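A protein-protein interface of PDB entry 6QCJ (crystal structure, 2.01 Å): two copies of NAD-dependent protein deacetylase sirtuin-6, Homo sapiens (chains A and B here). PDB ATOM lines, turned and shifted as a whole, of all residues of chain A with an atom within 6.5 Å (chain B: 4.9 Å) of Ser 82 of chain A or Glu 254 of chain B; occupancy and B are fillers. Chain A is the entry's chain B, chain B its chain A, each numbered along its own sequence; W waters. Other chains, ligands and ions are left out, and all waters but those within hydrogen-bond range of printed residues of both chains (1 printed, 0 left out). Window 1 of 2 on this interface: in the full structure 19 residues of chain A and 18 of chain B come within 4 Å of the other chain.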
ATOM      1  N   THR A  78     -17.921  15.963  10.857  1.00  0.00           N
ATOM      2  CA  THR A  78     -18.045  15.108   9.621  1.00  0.00           C
ATOM      3  C   THR A  78     -19.388  15.278   8.894  1.00  0.00           C
ATOM      4  O   THR A  78     -20.254  15.858   9.484  1.00  0.00           O
ATOM      5  CB  THR A  78     -17.977  13.595   9.897  1.00  0.00           C
ATOM      6  OG1 THR A  78     -18.290  12.897   8.693  1.00  0.00           O
ATOM      7  CG2 THR A  78     -18.945  13.154  10.967  1.00  0.00           C
ATOM      8  N   THR A  79     -19.577  14.592   7.753  1.00  0.00           N
ATOM      9  CA  THR A  79     -20.926  14.361   7.138  1.00  0.00           C
ATOM     10  C   THR A  79     -21.432  12.985   7.514  1.00  0.00           C
ATOM     11  O   THR A  79     -20.651  12.216   8.076  1.00  0.00           O
ATOM     12  CB  THR A  79     -20.878  14.535   5.637  1.00  0.00           C
ATOM     13  OG1 THR A  79     -20.006  13.535   5.123  1.00  0.00           O
ATOM     14  CG2 THR A  79     -20.401  15.933   5.352  1.00  0.00           C
ATOM     15  N   PHE A  80     -22.723  12.700   7.335  1.00  0.00           N
ATOM     16  CA  PHE A  80     -23.282  11.383   7.770  1.00  0.00           C
ATOM     17  C   PHE A  80     -22.707  10.245   6.916  1.00  0.00           C
ATOM     18  O   PHE A  80     -22.411   9.060   7.418  1.00  0.00           O
ATOM     19  CB  PHE A  80     -24.809  11.558   7.832  1.00  0.00           C
ATOM     20  CG  PHE A  80     -25.237  12.212   9.119  1.00  0.00           C
ATOM     21  CD1 PHE A  80     -25.118  11.529  10.316  1.00  0.00           C
ATOM     22  CD2 PHE A  80     -25.725  13.509   9.137  1.00  0.00           C
ATOM     23  CE1 PHE A  80     -25.527  12.115  11.506  1.00  0.00           C
ATOM     24  CE2 PHE A  80     -26.121  14.096  10.324  1.00  0.00           C
ATOM     25  CZ  PHE A  80     -26.021  13.400  11.508  1.00  0.00           C
ATOM     26  N   GLU A  81     -22.403  10.606   5.666  1.00  0.00           N
ATOM     27  CA  GLU A  81     -21.831   9.715   4.637  1.00  0.00           C
ATOM     28  C   GLU A  81     -20.377   9.392   4.972  1.00  0.00           C
ATOM     29  O   GLU A  81     -19.962   8.242   4.641  1.00  0.00           O
ATOM     30  CB  GLU A  81     -21.998  10.318   3.228  1.00  0.00           C
ATOM     31  CG  GLU A  81     -23.443  10.330   2.750  1.00  0.00           C
ATOM     32  CD  GLU A  81     -24.360  11.478   3.182  1.00  0.00           C
ATOM     33  OE1 GLU A  81     -23.834  12.483   3.731  1.00  0.00           O
ATOM     34  OE2 GLU A  81     -25.619  11.366   2.968  1.00  0.00           O
ATOM     35  N   SER A  82     -19.636  10.344   5.558  1.00  0.00           N
ATOM     36  CA  SER A  82     -18.173  10.225   5.791  1.00  0.00           C
ATOM     37  C   SER A  82     -17.912   9.710   7.207  1.00  0.00           C
ATOM     38  O   SER A  82     -16.802   9.233   7.450  1.00  0.00           O
ATOM     39  CB  SER A  82     -17.431  11.510   5.570  1.00  0.00           C
ATOM     40  OG  SER A  82     -17.725  12.066   4.297  1.00  0.00           O
ATOM     41  N   ALA A  83     -18.922   9.732   8.069  1.00  0.00           N
ATOM     42  CA  ALA A  83     -18.810   9.343   9.503  1.00  0.00           C
ATOM     43  C   ALA A  83     -18.282   7.908   9.583  1.00  0.00           C
ATOM     44  O   ALA A  83     -18.686   7.101   8.758  1.00  0.00           O
ATOM     45  CB  ALA A  83     -20.159   9.461  10.179  1.00  0.00           C
ATOM     46  N   ARG A  84     -17.340   7.606  10.474  1.00  0.00           N
ATOM     47  CA  ARG A  84     -16.878   6.206  10.583  1.00  0.00           C
ATOM     48  C   ARG A  84     -17.413   5.641  11.896  1.00  0.00           C
ATOM     49  O   ARG A  84     -17.365   6.298  12.925  1.00  0.00           O
ATOM     50  CB  ARG A  84     -15.370   6.077  10.344  1.00  0.00           C
ATOM     51  CG  ARG A  84     -14.470   6.645  11.424  1.00  0.00           C
ATOM     52  CD  ARG A  84     -13.144   5.901  11.342  1.00  0.00           C
ATOM     53  NE  ARG A  84     -13.285   4.534  11.828  1.00  0.00           N
ATOM     54  CZ  ARG A  84     -12.603   3.467  11.402  1.00  0.00           C
ATOM     55  NH1 ARG A  84     -11.704   3.585  10.440  1.00  0.00           N
ATOM     56  NH2 ARG A  84     -12.828   2.278  11.951  1.00  0.00           N
ATOM     57  N   ARG A 115     -24.190   0.553   8.893  1.00  0.00           N
ATOM     58  CA  ARG A 115     -22.969   0.763   8.072  1.00  0.00           C
ATOM     59  C   ARG A 115     -21.808  -0.061   8.648  1.00  0.00           C
ATOM     60  O   ARG A 115     -20.881  -0.391   7.878  1.00  0.00           O
ATOM     61  CB  ARG A 115     -22.785   2.260   7.923  1.00  0.00           C
ATOM     62  CG  ARG A 115     -23.660   2.805   6.802  1.00  0.00           C
ATOM     63  CD  ARG A 115     -24.081   4.263   6.894  1.00  0.00           C
ATOM     64  NE  ARG A 115     -23.093   5.167   6.296  1.00  0.00           N
ATOM     65  CZ  ARG A 115     -22.799   5.242   4.996  1.00  0.00           C
ATOM     66  NH1 ARG A 115     -23.451   4.485   4.145  1.00  0.00           N
ATOM     67  NH2 ARG A 115     -21.855   6.071   4.560  1.00  0.00           N
ATOM     68  N   PHE A 131     -30.573   6.908   6.160  1.00  0.00           N
ATOM     69  CA  PHE A 131     -30.194   6.237   4.891  1.00  0.00           C
ATOM     70  C   PHE A 131     -31.337   5.313   4.418  1.00  0.00           C
ATOM     71  O   PHE A 131     -31.171   4.701   3.345  1.00  0.00           O
ATOM     72  CB  PHE A 131     -28.903   5.429   5.109  1.00  0.00           C
ATOM     73  CG  PHE A 131     -27.679   6.250   5.482  1.00  0.00           C
ATOM     74  CD1 PHE A 131     -27.504   6.735   6.775  1.00  0.00           C
ATOM     75  CD2 PHE A 131     -26.742   6.606   4.533  1.00  0.00           C
ATOM     76  CE1 PHE A 131     -26.397   7.519   7.119  1.00  0.00           C
ATOM     77  CE2 PHE A 131     -25.638   7.400   4.863  1.00  0.00           C
ATOM     78  CZ  PHE A 131     -25.447   7.834   6.167  1.00  0.00           C
ATOM     79  N   TRP A 270     -13.110  -2.113  10.282  1.00  0.00           N
ATOM     80  CA  TRP A 270     -14.108  -1.575   9.316  1.00  0.00           C
ATOM     81  C   TRP A 270     -13.500  -1.441   7.910  1.00  0.00           C
ATOM     82  O   TRP A 270     -12.474  -0.753   7.748  1.00  0.00           O
ATOM     83  CB  TRP A 270     -14.658  -0.232   9.804  1.00  0.00           C
ATOM     84  CG  TRP A 270     -15.939   0.130   9.130  1.00  0.00           C
ATOM     85  CD1 TRP A 270     -17.110  -0.557   9.195  1.00  0.00           C
ATOM     86  CD2 TRP A 270     -16.218   1.303   8.345  1.00  0.00           C
ATOM     87  NE1 TRP A 270     -18.076   0.095   8.492  1.00  0.00           N
ATOM     88  CE2 TRP A 270     -17.592   1.259   8.017  1.00  0.00           C
ATOM     89  CE3 TRP A 270     -15.468   2.416   7.937  1.00  0.00           C
ATOM     90  CZ2 TRP A 270     -18.219   2.236   7.255  1.00  0.00           C
ATOM     91  CZ3 TRP A 270     -16.087   3.403   7.202  1.00  0.00           C
ATOM     92  CH2 TRP A 270     -17.436   3.305   6.849  1.00  0.00           C
ATOM     93  N   LEU B  24     -16.784  20.494  -5.402  1.00  0.00           N
ATOM     94  CA  LEU B  24     -15.971  19.697  -4.456  1.00  0.00           C
ATOM     95  C   LEU B  24     -15.385  18.546  -5.273  1.00  0.00           C
ATOM     96  O   LEU B  24     -14.156  18.447  -5.318  1.00  0.00           O
ATOM     97  CB  LEU B  24     -16.839  19.191  -3.298  1.00  0.00           C
ATOM     98  CG  LEU B  24     -16.059  18.544  -2.158  1.00  0.00           C
ATOM     99  CD1 LEU B  24     -15.044  19.520  -1.562  1.00  0.00           C
ATOM    100  CD2 LEU B  24     -16.997  18.029  -1.086  1.00  0.00           C
ATOM    101  N   GLN B  87      -9.555   8.568   9.493  1.00  0.00           N
ATOM    102  CA  GLN B  87      -9.340   8.311   8.033  1.00  0.00           C
ATOM    103  C   GLN B  87      -8.228   9.224   7.463  1.00  0.00           C
ATOM    104  O   GLN B  87      -7.334   8.733   6.870  1.00  0.00           O
ATOM    105  CB  GLN B  87     -10.649   8.453   7.261  1.00  0.00           C
ATOM    106  CG  GLN B  87     -11.701   7.447   7.760  1.00  0.00           C
ATOM    107  CD  GLN B  87     -13.095   7.636   7.200  1.00  0.00           C
ATOM    108  OE1 GLN B  87     -13.468   6.945   6.261  1.00  0.00           O
ATOM    109  NE2 GLN B  87     -13.846   8.615   7.698  1.00  0.00           N
ATOM    110  N   TYR B 251     -14.746  18.985   4.612  1.00  0.00           N
ATOM    111  CA  TYR B 251     -14.260  18.021   5.628  1.00  0.00           C
ATOM    112  C   TYR B 251     -13.081  17.278   5.059  1.00  0.00           C
ATOM    113  O   TYR B 251     -13.292  16.710   3.928  1.00  0.00           O
ATOM    114  CB  TYR B 251     -15.398  17.044   5.935  1.00  0.00           C
ATOM    115  CG  TYR B 251     -16.515  17.771   6.628  1.00  0.00           C
ATOM    116  CD1 TYR B 251     -16.339  18.276   7.912  1.00  0.00           C
ATOM    117  CD2 TYR B 251     -17.745  17.942   6.017  1.00  0.00           C
ATOM    118  CE1 TYR B 251     -17.380  18.914   8.583  1.00  0.00           C
ATOM    119  CE2 TYR B 251     -18.774  18.627   6.653  1.00  0.00           C
ATOM    120  CZ  TYR B 251     -18.609  19.080   7.950  1.00  0.00           C
ATOM    121  OH  TYR B 251     -19.646  19.762   8.550  1.00  0.00           O
ATOM    122  N   VAL B 252     -11.941  17.295   5.771  1.00  0.00           N
ATOM    123  CA  VAL B 252     -10.683  16.614   5.420  1.00  0.00           C
ATOM    124  C   VAL B 252     -10.923  15.122   5.138  1.00  0.00           C
ATOM    125  O   VAL B 252     -10.309  14.658   4.203  1.00  0.00           O
ATOM    126  CB  VAL B 252      -9.567  16.877   6.441  1.00  0.00           C
ATOM    127  CG1 VAL B 252      -9.153  18.323   6.279  1.00  0.00           C
ATOM    128  CG2 VAL B 252      -9.937  16.539   7.899  1.00  0.00           C
ATOM    129  N   ASP B 253     -11.879  14.443   5.802  1.00  0.00           N
ATOM    130  CA  ASP B 253     -12.068  12.957   5.659  1.00  0.00           C
ATOM    131  C   ASP B 253     -12.799  12.720   4.352  1.00  0.00           C
ATOM    132  O   ASP B 253     -12.383  11.855   3.646  1.00  0.00           O
ATOM    133  CB  ASP B 253     -12.823  12.266   6.806  1.00  0.00           C
ATOM    134  CG  ASP B 253     -12.038  12.059   8.073  1.00  0.00           C
ATOM    135  OD1 ASP B 253     -10.772  12.210   8.071  1.00  0.00           O
ATOM    136  OD2 ASP B 253     -12.661  11.687   9.079  1.00  0.00           O
ATOM    137  N   GLU B 254     -13.804  13.530   4.027  1.00  0.00           N
ATOM    138  CA  GLU B 254     -14.454  13.428   2.706  1.00  0.00           C
ATOM    139  C   GLU B 254     -13.392  13.757   1.633  1.00  0.00           C
ATOM    140  O   GLU B 254     -13.102  12.906   0.834  1.00  0.00           O
ATOM    141  CB  GLU B 254     -15.714  14.290   2.693  1.00  0.00           C
ATOM    142  CG  GLU B 254     -16.155  14.628   1.305  1.00  0.00           C
ATOM    143  CD  GLU B 254     -17.619  14.973   1.230  1.00  0.00           C
ATOM    144  OE1 GLU B 254     -18.029  15.894   1.977  1.00  0.00           O
ATOM    145  OE2 GLU B 254     -18.328  14.310   0.438  1.00  0.00           O
ATOM    146  N   VAL B 255     -12.755  14.928   1.687  1.00  0.00           N
ATOM    147  CA  VAL B 255     -11.626  15.201   0.760  1.00  0.00           C
ATOM    148  C   VAL B 255     -10.695  13.982   0.649  1.00  0.00           C
ATOM    149  O   VAL B 255     -10.478  13.530  -0.470  1.00  0.00           O
ATOM    150  CB  VAL B 255     -10.909  16.497   1.123  1.00  0.00           C
ATOM    151  CG1 VAL B 255      -9.587  16.648   0.394  1.00  0.00           C
ATOM    152  CG2 VAL B 255     -11.828  17.678   0.865  1.00  0.00           C
ATOM    153  N   MET B 256     -10.170  13.407   1.724  1.00  0.00           N
ATOM    154  CA  MET B 256      -9.028  12.465   1.572  1.00  0.00           C
ATOM    155  C   MET B 256      -9.493  11.069   1.131  1.00  0.00           C
ATOM    156  O   MET B 256      -8.745  10.458   0.406  1.00  0.00           O
ATOM    157  CB  MET B 256      -8.164  12.432   2.822  1.00  0.00           C
ATOM    158  CG  MET B 256      -7.489  13.772   3.092  1.00  0.00           C
ATOM    159  SD  MET B 256      -6.126  13.993   1.917  1.00  0.00           S
ATOM    160  CE  MET B 256      -4.934  12.818   2.470  1.00  0.00           C
ATOM    161  N   THR B 257     -10.735  10.639   1.369  1.00  0.00           N
ATOM    162  CA  THR B 257     -11.202   9.313   0.910  1.00  0.00           C
ATOM    163  C   THR B 257     -11.472   9.321  -0.617  1.00  0.00           C
ATOM    164  O   THR B 257     -11.136   8.338  -1.271  1.00  0.00           O
ATOM    165  CB  THR B 257     -12.381   8.898   1.802  1.00  0.00           C
ATOM    166  OG1 THR B 257     -13.411   9.828   1.584  1.00  0.00           O
ATOM    167  CG2 THR B 257     -12.094   8.981   3.290  1.00  0.00           C
ATOM    168  N   ARG B 258     -12.001  10.421  -1.192  1.00  0.00           N
ATOM    169  CA  ARG B 258     -12.208  10.668  -2.621  1.00  0.00           C
ATOM    170  C   ARG B 258     -10.832  10.682  -3.263  1.00  0.00           C
ATOM    171  O   ARG B 258     -10.648   9.971  -4.253  1.00  0.00           O
ATOM    172  CB  ARG B 258     -12.866  12.009  -2.895  1.00  0.00           C
ATOM    173  CG  ARG B 258     -14.354  12.001  -2.649  1.00  0.00           C
ATOM    174  CD  ARG B 258     -15.178  13.262  -2.642  1.00  0.00           C
ATOM    175  NE  ARG B 258     -16.425  12.517  -2.434  1.00  0.00           N
ATOM    176  CZ  ARG B 258     -17.646  12.794  -2.876  1.00  0.00           C
ATOM    177  NH1 ARG B 258     -17.917  13.921  -3.511  1.00  0.00           N
ATOM    178  NH2 ARG B 258     -18.616  11.925  -2.636  1.00  0.00           N
HETATM  179  O   HOH W   1     -15.073  11.130   9.485  1.00  0.00           O
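NE2 of Gln 87 of chain B lies within hydrogen-bond range of O of Ser 82 of chain A, at 3.0 Å.
The backbone NH (N) of Ala 83 of chain A lies within hydrogen-bond range of the side-chain hydroxyl (OG1) of Thr 78 of chain A, 3.3 Å away.
The guanidinium group (NE) of Arg 258 of chain B is in salt-bridge range of the side-chain carboxylate (OE2) of Glu 254 of chain B, 3.9 Å away.
OG of Ser 82 of chain A is in hydrogen-bond range of OG1 of Thr 79 of chain A, at 2.8 Å.
The side-chain hydroxyl of Thr 257 of chain B is in hydrogen-bond range of the backbone carbonyl oxygen of Glu 254 of chain B (3.2 Å).
Tyr 251 of chain B touches Thr 78 of chain A.
CD2 of Tyr 251 of chain B touches CG2 of Thr 79 of chain A (3.4 Å).
Ser 82 of chain A touches Glu 254 of chain B (OG to CB, 3.4 Å).
CB of Arg 84 of chain A touches NE2 of Gln 87 of chain B (3.97 Å).
Of the printed residues of chain B, Ser 82 of chain A touches Gln 87 (3.0 Å) and Glu 254 (3.4 Å).
Of chain A, only Ser 82 (3.4 Å) comes within 4 Å of Glu 254 of chain B.
Printed residues of chain B within 4 Å of Arg 84 of chain A: Gln 87 (3.97 Å).
Of the printed residues of chain A, Gln 87 of chain B touches Ser 82 and Arg 84.
Printed residues of chain B within 4 Å of Thr 79 of chain A: Tyr 251.
Val 252 of chain B touches none of the printed residues of chain A.
Val 255 of chain B touches none of the printed residues of chain A.
The nearest residue of chain B that does not touch Ser 82 of chain A is Asp 253 of chain B (4.8 Å).
The nearest residue of chain A that does not touch Glu 254 of chain B is Thr 79 of chain A (4.1 Å).
The nearest printed residue of chain A that does not touch Gln 87 of chain B is Trp 270 of chain A (4.5 Å).
Of the 10 printed residues of chain B, 3 touch a printed residue of chain A.
Printed residues of chain B that touch a printed residue of chain A: Gln 87, Tyr 251 and Glu 254.
Hydrophobic or aromatic side chains of chain B within 4 Å of the printed part of chain A: Tyr 251.
Along chain B the printed residues that touch a printed residue of chain A span positions 87 to 254.
Among the printed residues, 5 pairs touch across the chains.
Among the printed residues, no Asp or Glu carboxylate lies within 4 Å of a Lys or Arg side-chain nitrogen of the other chain.
No position is printed for both chains.
Water W1 lies within hydrogen-bond range of the side-chain carboxylate (OD2) of Asp 253 of chain B (2.5 Å), the backbone carbonyl oxygen (O) of Ser 82 of chain A (3.3 Å) and the side-chain amide nitrogen (NE2) of Gln 87 of chain B (3.3 Å).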
